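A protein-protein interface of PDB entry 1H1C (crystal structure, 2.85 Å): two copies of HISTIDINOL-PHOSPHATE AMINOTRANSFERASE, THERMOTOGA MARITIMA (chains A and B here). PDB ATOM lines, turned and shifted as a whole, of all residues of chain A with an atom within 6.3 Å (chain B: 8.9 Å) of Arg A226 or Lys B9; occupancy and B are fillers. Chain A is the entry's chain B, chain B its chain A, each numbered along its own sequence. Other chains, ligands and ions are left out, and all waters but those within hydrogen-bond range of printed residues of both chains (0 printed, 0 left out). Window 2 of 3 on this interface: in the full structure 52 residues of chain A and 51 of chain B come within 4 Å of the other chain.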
ATOM      1  N   MET A  95      -4.333  -0.660   0.757  1.00  0.00           N
ATOM      2  CA  MET A  95      -3.136  -1.427   0.521  1.00  0.00           C
ATOM      3  C   MET A  95      -2.563  -2.114   1.743  1.00  0.00           C
ATOM      4  O   MET A  95      -1.380  -2.426   1.772  1.00  0.00           O
ATOM      5  CB  MET A  95      -2.096  -0.515  -0.124  1.00  0.00           C
ATOM      6  CG  MET A  95      -2.144   0.892   0.411  1.00  0.00           C
ATOM      7  SD  MET A  95      -1.100   2.177  -0.577  1.00  0.00           S
ATOM      8  CE  MET A  95       0.522   1.154  -0.932  1.00  0.00           C
ATOM      9  N   ILE A 221       6.233   5.038  -1.696  1.00  0.00           N
ATOM     10  CA  ILE A 221       5.734   5.952  -2.698  1.00  0.00           C
ATOM     11  C   ILE A 221       5.543   5.249  -4.017  1.00  0.00           C
ATOM     12  O   ILE A 221       4.598   5.527  -4.747  1.00  0.00           O
ATOM     13  CB  ILE A 221       6.696   7.126  -2.886  1.00  0.00           C
ATOM     14  CG1 ILE A 221       6.929   7.800  -1.541  1.00  0.00           C
ATOM     15  CG2 ILE A 221       6.105   8.155  -3.829  1.00  0.00           C
ATOM     16  CD1 ILE A 221       5.640   8.206  -0.832  1.00  0.00           C
ATOM     17  N   ASP A 222       6.417   4.309  -4.328  1.00  0.00           N
ATOM     18  CA  ASP A 222       6.282   3.638  -5.603  1.00  0.00           C
ATOM     19  C   ASP A 222       5.027   2.784  -5.672  1.00  0.00           C
ATOM     20  O   ASP A 222       4.428   2.615  -6.738  1.00  0.00           O
ATOM     21  CB  ASP A 222       7.499   2.782  -5.907  1.00  0.00           C
ATOM     22  CG  ASP A 222       7.617   2.504  -7.374  1.00  0.00           C
ATOM     23  OD1 ASP A 222       7.864   3.480  -8.118  1.00  0.00           O
ATOM     24  OD2 ASP A 222       7.437   1.337  -7.792  1.00  0.00           O
ATOM     25  N   ALA A 223       4.644   2.249  -4.517  1.00  0.00           N
ATOM     26  CA  ALA A 223       3.464   1.416  -4.395  1.00  0.00           C
ATOM     27  C   ALA A 223       2.255   2.340  -4.366  1.00  0.00           C
ATOM     28  O   ALA A 223       1.364   2.236  -5.209  1.00  0.00           O
ATOM     29  CB  ALA A 223       3.540   0.621  -3.122  1.00  0.00           C
ATOM     30  N   TYR A 224       2.239   3.242  -3.385  1.00  0.00           N
ATOM     31  CA  TYR A 224       1.171   4.238  -3.213  1.00  0.00           C
ATOM     32  C   TYR A 224       0.692   4.830  -4.552  1.00  0.00           C
ATOM     33  O   TYR A 224      -0.513   4.850  -4.848  1.00  0.00           O
ATOM     34  CB  TYR A 224       1.671   5.380  -2.317  1.00  0.00           C
ATOM     35  CG  TYR A 224       0.736   6.571  -2.256  1.00  0.00           C
ATOM     36  CD1 TYR A 224      -0.501   6.477  -1.624  1.00  0.00           C
ATOM     37  CD2 TYR A 224       1.083   7.790  -2.836  1.00  0.00           C
ATOM     38  CE1 TYR A 224      -1.368   7.563  -1.573  1.00  0.00           C
ATOM     39  CE2 TYR A 224       0.216   8.876  -2.792  1.00  0.00           C
ATOM     40  CZ  TYR A 224      -1.012   8.754  -2.162  1.00  0.00           C
ATOM     41  OH  TYR A 224      -1.905   9.811  -2.164  1.00  0.00           O
ATOM     42  N   ASN A 225       1.640   5.321  -5.346  1.00  0.00           N
ATOM     43  CA  ASN A 225       1.330   5.909  -6.638  1.00  0.00           C
ATOM     44  C   ASN A 225       0.590   4.934  -7.556  1.00  0.00           C
ATOM     45  O   ASN A 225      -0.249   5.352  -8.353  1.00  0.00           O
ATOM     46  CB  ASN A 225       2.623   6.381  -7.307  1.00  0.00           C
ATOM     47  CG  ASN A 225       3.136   7.702  -6.741  1.00  0.00           C
ATOM     48  OD1 ASN A 225       4.327   8.030  -6.872  1.00  0.00           O
ATOM     49  ND2 ASN A 225       2.239   8.474  -6.121  1.00  0.00           N
ATOM     50  N   ARG A 226       0.892   3.643  -7.445  1.00  0.00           N
ATOM     51  CA  ARG A 226       0.253   2.628  -8.282  1.00  0.00           C
ATOM     52  C   ARG A 226      -1.215   2.383  -7.957  1.00  0.00           C
ATOM     53  O   ARG A 226      -1.989   1.960  -8.820  1.00  0.00           O
ATOM     54  CB  ARG A 226       0.985   1.288  -8.170  1.00  0.00           C
ATOM     55  CG  ARG A 226       2.404   1.340  -8.635  1.00  0.00           C
ATOM     56  CD  ARG A 226       3.040  -0.035  -8.673  1.00  0.00           C
ATOM     57  NE  ARG A 226       4.427   0.070  -9.124  1.00  0.00           N
ATOM     58  CZ  ARG A 226       5.155  -0.939  -9.591  1.00  0.00           C
ATOM     59  NH1 ARG A 226       6.404  -0.720  -9.969  1.00  0.00           N
ATOM     60  NH2 ARG A 226       4.644  -2.157  -9.692  1.00  0.00           N
ATOM     61  N   VAL A 227      -1.609   2.638  -6.719  1.00  0.00           N
ATOM     62  CA  VAL A 227      -2.988   2.381  -6.328  1.00  0.00           C
ATOM     63  C   VAL A 227      -3.851   3.619  -6.363  1.00  0.00           C
ATOM     64  O   VAL A 227      -5.069   3.510  -6.393  1.00  0.00           O
ATOM     65  CB  VAL A 227      -3.071   1.826  -4.895  1.00  0.00           C
ATOM     66  CG1 VAL A 227      -4.456   1.272  -4.633  1.00  0.00           C
ATOM     67  CG2 VAL A 227      -2.006   0.790  -4.680  1.00  0.00           C
ATOM     68  N   ARG A 228      -3.224   4.793  -6.334  1.00  0.00           N
ATOM     69  CA  ARG A 228      -3.986   6.027  -6.326  1.00  0.00           C
ATOM     70  C   ARG A 228      -4.342   6.440  -7.734  1.00  0.00           C
ATOM     71  O   ARG A 228      -3.662   6.049  -8.681  1.00  0.00           O
ATOM     72  CB  ARG A 228      -3.194   7.161  -5.642  1.00  0.00           C
ATOM     73  CG  ARG A 228      -2.057   7.753  -6.472  1.00  0.00           C
ATOM     74  CD  ARG A 228      -1.390   8.969  -5.811  1.00  0.00           C
ATOM     75  NE  ARG A 228      -0.221   9.419  -6.571  1.00  0.00           N
ATOM     76  CZ  ARG A 228      -0.266  10.067  -7.734  1.00  0.00           C
ATOM     77  NH1 ARG A 228       0.864  10.409  -8.333  1.00  0.00           N
ATOM     78  NH2 ARG A 228      -1.427  10.394  -8.290  1.00  0.00           N
ATOM     79  N   LEU B   6       7.442  -8.166   3.326  1.00  0.00           N
ATOM     80  CA  LEU B   6       6.960  -6.896   2.699  1.00  0.00           C
ATOM     81  C   LEU B   6       5.679  -7.079   1.884  1.00  0.00           C
ATOM     82  O   LEU B   6       5.028  -8.128   1.931  1.00  0.00           O
ATOM     83  CB  LEU B   6       8.054  -6.296   1.801  1.00  0.00           C
ATOM     84  CG  LEU B   6       9.266  -5.647   2.480  1.00  0.00           C
ATOM     85  CD1 LEU B   6       8.817  -4.424   3.281  1.00  0.00           C
ATOM     86  CD2 LEU B   6       9.971  -6.666   3.381  1.00  0.00           C
ATOM     87  N   ILE B   7       5.327  -6.031   1.146  1.00  0.00           N
ATOM     88  CA  ILE B   7       4.141  -6.045   0.313  1.00  0.00           C
ATOM     89  C   ILE B   7       4.424  -5.395  -1.052  1.00  0.00           C
ATOM     90  O   ILE B   7       4.118  -4.221  -1.302  1.00  0.00           O
ATOM     91  CB  ILE B   7       2.970  -5.352   1.042  1.00  0.00           C
ATOM     92  CG1 ILE B   7       1.670  -5.594   0.274  1.00  0.00           C
ATOM     93  CG2 ILE B   7       3.269  -3.860   1.230  1.00  0.00           C
ATOM     94  CD1 ILE B   7       0.413  -5.254   1.076  1.00  0.00           C
ATOM     95  N   ALA B   8       5.043  -6.192  -1.921  1.00  0.00           N
ATOM     96  CA  ALA B   8       5.384  -5.782  -3.273  1.00  0.00           C
ATOM     97  C   ALA B   8       4.258  -6.208  -4.205  1.00  0.00           C
ATOM     98  O   ALA B   8       3.689  -7.294  -4.066  1.00  0.00           O
ATOM     99  CB  ALA B   8       6.688  -6.422  -3.703  1.00  0.00           C
ATOM    100  N   LYS B   9       3.945  -5.336  -5.156  1.00  0.00           N
ATOM    101  CA  LYS B   9       2.882  -5.585  -6.113  1.00  0.00           C
ATOM    102  C   LYS B   9       3.371  -5.666  -7.555  1.00  0.00           C
ATOM    103  O   LYS B   9       4.349  -5.020  -7.941  1.00  0.00           O
ATOM    104  CB  LYS B   9       1.819  -4.501  -5.974  1.00  0.00           C
ATOM    105  CG  LYS B   9       2.396  -3.110  -5.801  1.00  0.00           C
ATOM    106  CD  LYS B   9       1.484  -2.261  -4.930  1.00  0.00           C
ATOM    107  CE  LYS B   9       1.326  -2.886  -3.545  1.00  0.00           C
ATOM    108  NZ  LYS B   9       0.481  -2.070  -2.630  1.00  0.00           N
ATOM    109  N   ARG B  10       2.659  -6.472  -8.336  1.00  0.00           N
ATOM    110  CA  ARG B  10       2.960  -6.709  -9.741  1.00  0.00           C
ATOM    111  C   ARG B  10       2.318  -5.656 -10.643  1.00  0.00           C
ATOM    112  O   ARG B  10       2.771  -5.435 -11.768  1.00  0.00           O
ATOM    113  CB  ARG B  10       2.460  -8.096 -10.137  1.00  0.00           C
ATOM    114  CG  ARG B  10       0.934  -8.251 -10.104  1.00  0.00           C
ATOM    115  CD  ARG B  10       0.325  -8.119  -8.696  1.00  0.00           C
ATOM    116  NE  ARG B  10       0.725  -9.200  -7.786  1.00  0.00           N
ATOM    117  CZ  ARG B  10       0.150  -9.458  -6.610  1.00  0.00           C
ATOM    118  NH1 ARG B  10      -0.867  -8.720  -6.178  1.00  0.00           N
ATOM    119  NH2 ARG B  10       0.597 -10.457  -5.853  1.00  0.00           N
ATOM    120  N   ALA B  11       1.256  -5.027 -10.144  1.00  0.00           N
ATOM    121  CA  ALA B  11       0.541  -3.980 -10.869  1.00  0.00           C
ATOM    122  C   ALA B  11       1.487  -3.082 -11.673  1.00  0.00           C
ATOM    123  O   ALA B  11       2.654  -2.932 -11.327  1.00  0.00           O
ATOM    124  CB  ALA B  11      -0.247  -3.142  -9.884  1.00  0.00           C
ATOM    125  N   TYR B  12       0.975  -2.482 -12.745  1.00  0.00           N
ATOM    126  CA  TYR B  12       1.781  -1.605 -13.594  1.00  0.00           C
ATOM    127  C   TYR B  12       2.272  -0.385 -12.838  1.00  0.00           C
ATOM    128  O   TYR B  12       1.508   0.267 -12.125  1.00  0.00           O
ATOM    129  CB  TYR B  12       0.983  -1.150 -14.815  1.00  0.00           C
ATOM    130  CG  TYR B  12       0.471  -2.304 -15.638  1.00  0.00           C
ATOM    131  CD1 TYR B  12      -0.856  -2.723 -15.542  1.00  0.00           C
ATOM    132  CD2 TYR B  12       1.327  -3.007 -16.485  1.00  0.00           C
ATOM    133  CE1 TYR B  12      -1.320  -3.820 -16.271  1.00  0.00           C
ATOM    134  CE2 TYR B  12       0.878  -4.103 -17.215  1.00  0.00           C
ATOM    135  CZ  TYR B  12      -0.445  -4.505 -17.103  1.00  0.00           C
ATOM    136  OH  TYR B  12      -0.890  -5.598 -17.814  1.00  0.00           O
ATOM    137  N   PRO B  13       3.562  -0.054 -12.996  1.00  0.00           N
ATOM    138  CA  PRO B  13       4.171   1.097 -12.326  1.00  0.00           C
ATOM    139  C   PRO B  13       3.520   2.411 -12.709  1.00  0.00           C
ATOM    140  O   PRO B  13       2.840   2.511 -13.733  1.00  0.00           O
ATOM    141  CB  PRO B  13       5.627   1.025 -12.777  1.00  0.00           C
ATOM    142  CG  PRO B  13       5.524   0.430 -14.143  1.00  0.00           C
ATOM    143  CD  PRO B  13       4.506  -0.665 -13.948  1.00  0.00           C
ATOM    144  N   TYR B  14       3.731   3.421 -11.880  1.00  0.00           N
ATOM    145  CA  TYR B  14       3.181   4.736 -12.148  1.00  0.00           C
ATOM    146  C   TYR B  14       4.178   5.516 -13.006  1.00  0.00           C
ATOM    147  O   TYR B  14       5.387   5.461 -12.775  1.00  0.00           O
ATOM    148  CB  TYR B  14       2.925   5.454 -10.832  1.00  0.00           C
ATOM    149  CG  TYR B  14       2.791   6.943 -10.970  1.00  0.00           C
ATOM    150  CD1 TYR B  14       1.603   7.524 -11.387  1.00  0.00           C
ATOM    151  CD2 TYR B  14       3.867   7.778 -10.686  1.00  0.00           C
ATOM    152  CE1 TYR B  14       1.490   8.904 -11.513  1.00  0.00           C
ATOM    153  CE2 TYR B  14       3.765   9.149 -10.814  1.00  0.00           C
ATOM    154  CZ  TYR B  14       2.578   9.708 -11.227  1.00  0.00           C
ATOM    155  OH  TYR B  14       2.483  11.075 -11.358  1.00  0.00           O
ATOM    156  N   GLU B  15       3.672   6.236 -14.001  1.00  0.00           N
ATOM    157  CA  GLU B  15       4.526   7.012 -14.899  1.00  0.00           C
ATOM    158  C   GLU B  15       3.776   8.277 -15.310  1.00  0.00           C
ATOM    159  O   GLU B  15       2.652   8.512 -14.865  1.00  0.00           O
ATOM    160  CB  GLU B  15       4.853   6.186 -16.156  1.00  0.00           C
ATOM    161  CG  GLU B  15       5.153   4.703 -15.892  1.00  0.00           C
ATOM    162  CD  GLU B  15       5.180   3.851 -17.161  1.00  0.00           C
ATOM    163  OE1 GLU B  15       5.322   2.610 -17.044  1.00  0.00           O
ATOM    164  OE2 GLU B  15       5.057   4.417 -18.272  1.00  0.00           O
ATOM    165  N   TYR B  90     -13.407   4.569  -9.963  1.00  0.00           N
ATOM    166  CA  TYR B  90     -12.623   4.076  -8.859  1.00  0.00           C
ATOM    167  C   TYR B  90     -13.511   3.684  -7.687  1.00  0.00           C
ATOM    168  O   TYR B  90     -13.614   2.507  -7.368  1.00  0.00           O
ATOM    169  CB  TYR B  90     -11.628   5.148  -8.455  1.00  0.00           C
ATOM    170  CG  TYR B  90     -10.466   4.685  -7.633  1.00  0.00           C
ATOM    171  CD1 TYR B  90     -10.413   4.944  -6.265  1.00  0.00           C
ATOM    172  CD2 TYR B  90      -9.374   4.061  -8.234  1.00  0.00           C
ATOM    173  CE1 TYR B  90      -9.300   4.601  -5.520  1.00  0.00           C
ATOM    174  CE2 TYR B  90      -8.249   3.713  -7.495  1.00  0.00           C
ATOM    175  CZ  TYR B  90      -8.219   3.988  -6.143  1.00  0.00           C
ATOM    176  OH  TYR B  90      -7.100   3.684  -5.407  1.00  0.00           O
ATOM    177  N   ILE B 111      -6.964  -1.524 -15.007  1.00  0.00           N
ATOM    178  CA  ILE B 111      -5.963  -0.995 -14.101  1.00  0.00           C
ATOM    179  C   ILE B 111      -6.549  -0.635 -12.748  1.00  0.00           C
ATOM    180  O   ILE B 111      -6.025  -1.017 -11.710  1.00  0.00           O
ATOM    181  CB  ILE B 111      -5.349   0.288 -14.617  1.00  0.00           C
ATOM    182  CG1 ILE B 111      -4.741   0.071 -16.008  1.00  0.00           C
ATOM    183  CG2 ILE B 111      -4.378   0.823 -13.571  1.00  0.00           C
ATOM    184  CD1 ILE B 111      -3.774  -1.094 -16.117  1.00  0.00           C
ATOM    185  N   PHE B 112      -7.617   0.149 -12.760  1.00  0.00           N
ATOM    186  CA  PHE B 112      -8.245   0.547 -11.522  1.00  0.00           C
ATOM    187  C   PHE B 112      -8.692  -0.678 -10.773  1.00  0.00           C
ATOM    188  O   PHE B 112      -8.499  -0.780  -9.567  1.00  0.00           O
ATOM    189  CB  PHE B 112      -9.428   1.451 -11.802  1.00  0.00           C
ATOM    190  CG  PHE B 112      -9.036   2.838 -12.196  1.00  0.00           C
ATOM    191  CD1 PHE B 112      -7.720   3.259 -12.055  1.00  0.00           C
ATOM    192  CD2 PHE B 112      -9.978   3.723 -12.705  1.00  0.00           C
ATOM    193  CE1 PHE B 112      -7.343   4.527 -12.413  1.00  0.00           C
ATOM    194  CE2 PHE B 112      -9.608   5.004 -13.070  1.00  0.00           C
ATOM    195  CZ  PHE B 112      -8.283   5.406 -12.922  1.00  0.00           C
ATOM    196  N   ALA B 113      -9.287  -1.610 -11.507  1.00  0.00           N
ATOM    197  CA  ALA B 113      -9.749  -2.868 -10.939  1.00  0.00           C
ATOM    198  C   ALA B 113      -8.684  -3.429 -10.009  1.00  0.00           C
ATOM    199  O   ALA B 113      -8.973  -3.734  -8.858  1.00  0.00           O
ATOM    200  CB  ALA B 113     -10.043  -3.868 -12.051  1.00  0.00           C
ATOM    201  N   LYS B 114      -7.454  -3.557 -10.502  1.00  0.00           N
ATOM    202  CA  LYS B 114      -6.370  -4.088  -9.686  1.00  0.00           C
ATOM    203  C   LYS B 114      -5.920  -3.197  -8.532  1.00  0.00           C
ATOM    204  O   LYS B 114      -5.615  -3.696  -7.455  1.00  0.00           O
ATOM    205  CB  LYS B 114      -5.162  -4.430 -10.551  1.00  0.00           C
ATOM    206  CG  LYS B 114      -5.311  -5.696 -11.379  1.00  0.00           C
ATOM    207  CD  LYS B 114      -4.064  -5.902 -12.238  1.00  0.00           C
ATOM    208  CE  LYS B 114      -3.991  -7.309 -12.811  1.00  0.00           C
ATOM    209  NZ  LYS B 114      -5.085  -7.587 -13.792  1.00  0.00           N
ATOM    210  N   ALA B 115      -5.865  -1.887  -8.736  1.00  0.00           N
ATOM    211  CA  ALA B 115      -5.437  -1.015  -7.648  1.00  0.00           C
ATOM    212  C   ALA B 115      -6.350  -1.217  -6.430  1.00  0.00           C
ATOM    213  O   ALA B 115      -5.884  -1.474  -5.311  1.00  0.00           O
ATOM    214  CB  ALA B 115      -5.461   0.463  -8.093  1.00  0.00           C
ATOM    215  N   VAL B 116      -7.653  -1.117  -6.668  1.00  0.00           N
ATOM    216  CA  VAL B 116      -8.647  -1.256  -5.620  1.00  0.00           C
ATOM    217  C   VAL B 116      -8.736  -2.665  -5.047  1.00  0.00           C
ATOM    218  O   VAL B 116      -9.003  -2.857  -3.857  1.00  0.00           O
ATOM    219  CB  VAL B 116     -10.037  -0.832  -6.153  1.00  0.00           C
ATOM    220  CG1 VAL B 116     -11.143  -1.374  -5.264  1.00  0.00           C
ATOM    221  CG2 VAL B 116     -10.126   0.685  -6.196  1.00  0.00           C
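The backbone carbonyl oxygen (O) of Lys B9 sits at hydrogen-bond distance from the guanidinium group (NH2) of Arg A226, 3.4 Å away. NH2 of Arg A226 is in hydrogen-bond range of O of Ala B11. OH of Tyr B14 sits close to NH1 of Arg A228, at 3.5 Å. The backbone carbonyl oxygen (O) of Val A227 lies close to the side-chain hydroxyl (OH) of Tyr B90 (2.3 Å).
O of Ile A221 sits close to OD1 of Asn A225 (3.3 Å). The guanidinium group (NH1) of Arg A226 is in salt-bridge range of the side-chain carboxylate (OD2) of Asp A222 (3.2 Å). ND2 of Asn A225 lies close to NE of Arg A228 (2.7 Å).
O of Met A95 touches CD1 of Ile B7 (3.4 Å). Met A95 touches Lys B9 (CE to NZ, 3.6 Å). Ala A223 touches Lys B9. Tyr B14 touches Asn A225 (CB to CB, 3.7 Å). Arg A226 touches Tyr B12 (CG to O, 3.8 Å). CA of Pro B13 touches NE of Arg A226 (3.4 Å). O of Arg A226 touches CB of Ala B115, at 3.9 Å. Ala B115 touches Val A227 (O to CG1, 3.2 Å).
Of chain B, only Lys B9, Ala B11, Tyr B12, Pro B13 and Ala B115 come within 4 Å of Arg A226. Of the printed residues of chain A, Lys B9 touches Met A95 (3.6 Å), Ala A223 (3.98 Å) and Arg A226 (3.4 Å). Ala A223 touches just one residue of chain B: Lys B9. Of chain B, only Tyr B90 (2.3 Å) and Ala B115 (3.2 Å) come within 4 Å of Val A227. Of the printed residues of chain A, Tyr B90 touches Val A227. Printed residues of chain A within 4 Å of Ala B115: Arg A226 and Val A227. Printed residues of chain A within 4 Å of Tyr B14: Asn A225 (3.7 Å) and Arg A228 (3.4 Å). Of the printed residues of chain A, Ile B7 touches Met A95 (3.4 Å). Val B116 touches none of the printed residues of chain A. Ile B111 touches none of the printed residues of chain A. The nearest printed residue of chain A that does not touch Pro B13 is Asp A222 (5.3 Å).
Hydrophobic or aromatic side chains of chain A within 4 Å of the printed part of chain B: Met A95, Ala A223 and Val A227. Of the 17 printed residues of chain B, 8 touch a printed residue of chain A. Along chain B the printed residues that touch a printed residue of chain A span positions 7 to 115.
No position is printed for both chains. Of the 12 pairs that touch across the chains among the printed residues, none has its exchanged pair printed and touching as well.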
